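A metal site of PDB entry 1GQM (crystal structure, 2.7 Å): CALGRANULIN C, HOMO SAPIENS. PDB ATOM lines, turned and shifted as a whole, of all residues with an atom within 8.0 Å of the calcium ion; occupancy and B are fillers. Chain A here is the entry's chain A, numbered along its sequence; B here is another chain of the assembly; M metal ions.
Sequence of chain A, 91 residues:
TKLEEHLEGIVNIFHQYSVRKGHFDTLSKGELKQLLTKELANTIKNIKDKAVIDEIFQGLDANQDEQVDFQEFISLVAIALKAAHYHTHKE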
ATOM      1  N   THR A  26      29.225  -7.562   4.343  1.00  0.00           N
ATOM      2  CA  THR A  26      28.168  -8.443   4.843  1.00  0.00           C
ATOM      3  C   THR A  26      27.019  -7.661   5.456  1.00  0.00           C
ATOM      4  O   THR A  26      27.158  -6.431   5.711  1.00  0.00           O
ATOM      5  CB  THR A  26      28.734  -9.435   5.878  1.00  0.00           C
ATOM      6  OG1 THR A  26      29.500  -8.722   6.877  1.00  0.00           O
ATOM      7  CG2 THR A  26      29.784 -10.337   5.201  1.00  0.00           C
ATOM      8  N   LEU A  27      25.906  -8.355   5.676  1.00  0.00           N
ATOM      9  CA  LEU A  27      24.672  -7.798   6.205  1.00  0.00           C
ATOM     10  C   LEU A  27      24.412  -8.259   7.624  1.00  0.00           C
ATOM     11  O   LEU A  27      24.343  -9.460   7.905  1.00  0.00           O
ATOM     12  CB  LEU A  27      23.492  -8.295   5.376  1.00  0.00           C
ATOM     13  CG  LEU A  27      23.399  -7.794   3.946  1.00  0.00           C
ATOM     14  CD1 LEU A  27      22.593  -8.751   3.093  1.00  0.00           C
ATOM     15  CD2 LEU A  27      22.803  -6.363   3.935  1.00  0.00           C
ATOM     16  N   PHE A  57      16.362 -14.313   8.595  1.00  0.00           N
ATOM     17  CA  PHE A  57      17.757 -14.199   8.921  1.00  0.00           C
ATOM     18  C   PHE A  57      18.347 -15.573   9.331  1.00  0.00           C
ATOM     19  O   PHE A  57      19.353 -16.019   8.770  1.00  0.00           O
ATOM     20  CB  PHE A  57      17.931 -13.215  10.052  1.00  0.00           C
ATOM     21  CG  PHE A  57      19.334 -13.062  10.496  1.00  0.00           C
ATOM     22  CD1 PHE A  57      20.221 -12.308   9.780  1.00  0.00           C
ATOM     23  CD2 PHE A  57      19.783 -13.694  11.619  1.00  0.00           C
ATOM     24  CE1 PHE A  57      21.530 -12.144  10.200  1.00  0.00           C
ATOM     25  CE2 PHE A  57      21.107 -13.520  12.053  1.00  0.00           C
ATOM     26  CZ  PHE A  57      21.976 -12.750  11.345  1.00  0.00           C
ATOM     27  N   LEU A  60      19.062 -17.735   6.256  1.00  0.00           N
ATOM     28  CA  LEU A  60      20.131 -17.379   5.380  1.00  0.00           C
ATOM     29  C   LEU A  60      21.505 -17.485   6.021  1.00  0.00           C
ATOM     30  O   LEU A  60      22.505 -17.679   5.314  1.00  0.00           O
ATOM     31  CB  LEU A  60      19.947 -15.965   4.874  1.00  0.00           C
ATOM     32  CG  LEU A  60      18.713 -15.625   4.015  1.00  0.00           C
ATOM     33  CD1 LEU A  60      18.603 -14.136   3.810  1.00  0.00           C
ATOM     34  CD2 LEU A  60      18.735 -16.347   2.665  1.00  0.00           C
ATOM     35  N   ASP A  61      21.592 -17.363   7.354  1.00  0.00           N
ATOM     36  CA  ASP A  61      22.917 -17.371   7.991  1.00  0.00           C
ATOM     37  C   ASP A  61      23.429 -18.754   8.419  1.00  0.00           C
ATOM     38  O   ASP A  61      23.556 -19.074   9.601  1.00  0.00           O
ATOM     39  CB  ASP A  61      22.916 -16.409   9.152  1.00  0.00           C
ATOM     40  CG  ASP A  61      24.202 -16.412   9.880  1.00  0.00           C
ATOM     41  OD1 ASP A  61      25.249 -16.622   9.216  1.00  0.00           O
ATOM     42  OD2 ASP A  61      24.244 -16.215  11.113  1.00  0.00           O
ATOM     43  N   ALA A  62      23.735 -19.535   7.406  1.00  0.00           N
ATOM     44  CA  ALA A  62      24.139 -20.941   7.488  1.00  0.00           C
ATOM     45  C   ALA A  62      25.366 -21.261   8.283  1.00  0.00           C
ATOM     46  O   ALA A  62      25.463 -22.389   8.771  1.00  0.00           O
ATOM     47  CB  ALA A  62      24.316 -21.517   6.063  1.00  0.00           C
ATOM     48  N   ASN A  63      26.320 -20.340   8.381  1.00  0.00           N
ATOM     49  CA  ASN A  63      27.524 -20.633   9.187  1.00  0.00           C
ATOM     50  C   ASN A  63      27.429 -20.103  10.601  1.00  0.00           C
ATOM     51  O   ASN A  63      28.366 -20.269  11.386  1.00  0.00           O
ATOM     52  CB  ASN A  63      28.826 -20.210   8.516  1.00  0.00           C
ATOM     53  CG  ASN A  63      28.894 -18.745   8.244  1.00  0.00           C
ATOM     54  OD1 ASN A  63      27.996 -17.982   8.613  1.00  0.00           O
ATOM     55  ND2 ASN A  63      29.963 -18.314   7.622  1.00  0.00           N
ATOM     56  N   GLN A  64      26.295 -19.480  10.915  1.00  0.00           N
ATOM     57  CA  GLN A  64      25.988 -18.989  12.279  1.00  0.00           C
ATOM     58  C   GLN A  64      26.941 -17.930  12.757  1.00  0.00           C
ATOM     59  O   GLN A  64      27.268 -17.881  13.932  1.00  0.00           O
ATOM     60  CB  GLN A  64      26.014 -20.119  13.331  1.00  0.00           C
ATOM     61  CG  GLN A  64      25.022 -21.242  13.119  1.00  0.00           C
ATOM     62  CD  GLN A  64      23.583 -20.798  13.173  1.00  0.00           C
ATOM     63  OE1 GLN A  64      23.236 -19.742  13.738  1.00  0.00           O
ATOM     64  NE2 GLN A  64      22.714 -21.642  12.611  1.00  0.00           N
ATOM     65  N   ASP A  65      27.398 -17.099  11.849  1.00  0.00           N
ATOM     66  CA  ASP A  65      28.367 -16.094  12.217  1.00  0.00           C
ATOM     67  C   ASP A  65      27.658 -14.768  12.399  1.00  0.00           C
ATOM     68  O   ASP A  65      28.292 -13.732  12.373  1.00  0.00           O
ATOM     69  CB  ASP A  65      29.409 -15.983  11.120  1.00  0.00           C
ATOM     70  CG  ASP A  65      28.854 -15.365   9.857  1.00  0.00           C
ATOM     71  OD1 ASP A  65      27.634 -15.422   9.615  1.00  0.00           O
ATOM     72  OD2 ASP A  65      29.577 -14.798   9.035  1.00  0.00           O
ATOM     73  N   GLU A  66      26.350 -14.830  12.566  1.00  0.00           N
ATOM     74  CA  GLU A  66      25.511 -13.673  12.761  1.00  0.00           C
ATOM     75  C   GLU A  66      25.687 -12.687  11.636  1.00  0.00           C
ATOM     76  O   GLU A  66      25.436 -11.492  11.819  1.00  0.00           O
ATOM     77  CB  GLU A  66      25.784 -13.003  14.115  1.00  0.00           C
ATOM     78  CG  GLU A  66      25.462 -13.848  15.341  1.00  0.00           C
ATOM     79  CD  GLU A  66      24.027 -14.334  15.356  1.00  0.00           C
ATOM     80  OE1 GLU A  66      23.217 -13.705  14.651  1.00  0.00           O
ATOM     81  OE2 GLU A  66      23.690 -15.329  16.053  1.00  0.00           O
ATOM     82  N   GLN A  67      26.158 -13.145  10.490  1.00  0.00           N
ATOM     83  CA  GLN A  67      26.176 -12.261   9.338  1.00  0.00           C
ATOM     84  C   GLN A  67      25.648 -12.955   8.103  1.00  0.00           C
ATOM     85  O   GLN A  67      25.649 -14.194   8.004  1.00  0.00           O
ATOM     86  CB  GLN A  67      27.549 -11.682   9.043  1.00  0.00           C
ATOM     87  CG  GLN A  67      28.210 -10.909  10.194  1.00  0.00           C
ATOM     88  CD  GLN A  67      27.748  -9.456  10.332  1.00  0.00           C
ATOM     89  OE1 GLN A  67      27.605  -8.748   9.342  1.00  0.00           O
ATOM     90  NE2 GLN A  67      27.548  -9.014  11.562  1.00  0.00           N
ATOM     91  N   VAL A  68      25.179 -12.170   7.156  1.00  0.00           N
ATOM     92  CA  VAL A  68      24.718 -12.776   5.939  1.00  0.00           C
ATOM     93  C   VAL A  68      25.627 -12.276   4.882  1.00  0.00           C
ATOM     94  O   VAL A  68      25.578 -11.097   4.584  1.00  0.00           O
ATOM     95  CB  VAL A  68      23.324 -12.366   5.624  1.00  0.00           C
ATOM     96  CG1 VAL A  68      22.952 -12.775   4.175  1.00  0.00           C
ATOM     97  CG2 VAL A  68      22.391 -13.030   6.590  1.00  0.00           C
ATOM     98  N   ASP A  69      26.474 -13.180   4.348  1.00  0.00           N
ATOM     99  CA  ASP A  69      27.420 -12.888   3.253  1.00  0.00           C
ATOM    100  C   ASP A  69      26.833 -13.115   1.849  1.00  0.00           C
ATOM    101  O   ASP A  69      25.782 -13.742   1.688  1.00  0.00           O
ATOM    102  CB  ASP A  69      28.754 -13.625   3.430  1.00  0.00           C
ATOM    103  CG  ASP A  69      28.648 -15.148   3.270  1.00  0.00           C
ATOM    104  OD1 ASP A  69      27.788 -15.614   2.460  1.00  0.00           O
ATOM    105  OD2 ASP A  69      29.377 -15.969   3.887  1.00  0.00           O
ATOM    106  N   PHE A  70      27.506 -12.610   0.818  1.00  0.00           N
ATOM    107  CA  PHE A  70      26.867 -12.656  -0.515  1.00  0.00           C
ATOM    108  C   PHE A  70      26.408 -14.069  -0.937  1.00  0.00           C
ATOM    109  O   PHE A  70      25.289 -14.229  -1.420  1.00  0.00           O
ATOM    110  CB  PHE A  70      27.681 -11.975  -1.607  1.00  0.00           C
ATOM    111  CG  PHE A  70      26.868 -11.718  -2.858  1.00  0.00           C
ATOM    112  CD1 PHE A  70      25.858 -10.766  -2.872  1.00  0.00           C
ATOM    113  CD2 PHE A  70      27.084 -12.453  -4.012  1.00  0.00           C
ATOM    114  CE1 PHE A  70      25.110 -10.566  -4.035  1.00  0.00           C
ATOM    115  CE2 PHE A  70      26.331 -12.232  -5.140  1.00  0.00           C
ATOM    116  CZ  PHE A  70      25.358 -11.299  -5.152  1.00  0.00           C
ATOM    117  N   GLU A  72      25.397 -16.379   0.833  1.00  0.00           N
ATOM    118  CA  GLU A  72      24.232 -16.841   1.553  1.00  0.00           C
ATOM    119  C   GLU A  72      23.073 -16.072   1.016  1.00  0.00           C
ATOM    120  O   GLU A  72      21.969 -16.590   1.003  1.00  0.00           O
ATOM    121  CB  GLU A  72      24.352 -16.649   3.072  1.00  0.00           C
ATOM    122  CG  GLU A  72      25.673 -17.102   3.675  1.00  0.00           C
ATOM    123  CD  GLU A  72      25.767 -16.868   5.171  1.00  0.00           C
ATOM    124  OE1 GLU A  72      25.949 -15.696   5.591  1.00  0.00           O
ATOM    125  OE2 GLU A  72      25.711 -17.855   5.931  1.00  0.00           O
ATOM    126  N   LYS B  45      30.947 -19.460  15.888  1.00  0.00           N
ATOM    127  CA  LYS B  45      30.792 -18.452  16.939  1.00  0.00           C
ATOM    128  C   LYS B  45      29.660 -18.720  17.911  1.00  0.00           C
ATOM    129  O   LYS B  45      28.602 -19.260  17.548  1.00  0.00           O
ATOM    130  CB  LYS B  45      30.769 -17.045  16.375  1.00  0.00           C
ATOM    131  CG  LYS B  45      30.779 -17.019  14.866  1.00  0.00           C
ATOM    132  CD  LYS B  45      32.077 -17.576  14.230  1.00  0.00           C
ATOM    133  CE  LYS B  45      31.751 -18.346  12.896  1.00  0.00           C
ATOM    134  NZ  LYS B  45      32.879 -18.275  11.911  1.00  0.00           N
ATOM    135  N   LYS B  82      33.575 -24.514   6.195  1.00  0.00           N
ATOM    136  CA  LYS B  82      33.519 -23.217   5.592  1.00  0.00           C
ATOM    137  C   LYS B  82      34.216 -22.269   6.524  1.00  0.00           C
ATOM    138  O   LYS B  82      34.946 -21.333   6.090  1.00  0.00           O
ATOM    139  CB  LYS B  82      32.099 -22.755   5.346  1.00  0.00           C
ATOM    140  CG  LYS B  82      32.039 -21.556   4.413  1.00  0.00           C
ATOM    141  CD  LYS B  82      30.638 -21.344   3.872  1.00  0.00           C
HETATM  142 CA    CA M   1      27.092 -15.995   7.660  1.00  0.00          CA
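The side-chain amide oxygen (OE1) of Gln 67 sits at hydrogen-bond distance from the side-chain hydroxyl (OG1) of Thr 26 (3.1 Å).
N of Glu 72 sits close to OD1 of Asp 69 (3.0 Å).
N of Ala 62 lies close to OE2 of Glu 72, 3.0 Å away.
OD1 of Asp 61 lies close to N of Gln 64 (3.5 Å).
OD2 of Asp 61 sits at hydrogen-bond distance from N of Glu 66.
The calcium ion is bound by the side-chain carboxylate (OD1) of Asp 65 (2.1 Å), the backbone carbonyl oxygen (O) of Gln 67 (2.3 Å), the side-chain amide oxygen (OD1) of Asn 63 (2.4 Å), the side-chain carboxylate (OE1) of Glu 72 (2.4 Å), the side-chain carboxylate (OD1) of Asp 61 (2.5 Å) and the side-chain carboxylate (OE2) of Glu 72 (2.9 Å).
The calcium ion has six donor atoms within binding distance.
Slightly farther from the calcium ion lies OD2 of Asp 65 (3.1 Å).
Within 4 Å of the calcium ion: Asp 61, Asn 63, Asp 65, Gln 67 and Glu 72.
Along chain A the residues within 4 Å of the calcium ion span positions 61 to 72.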
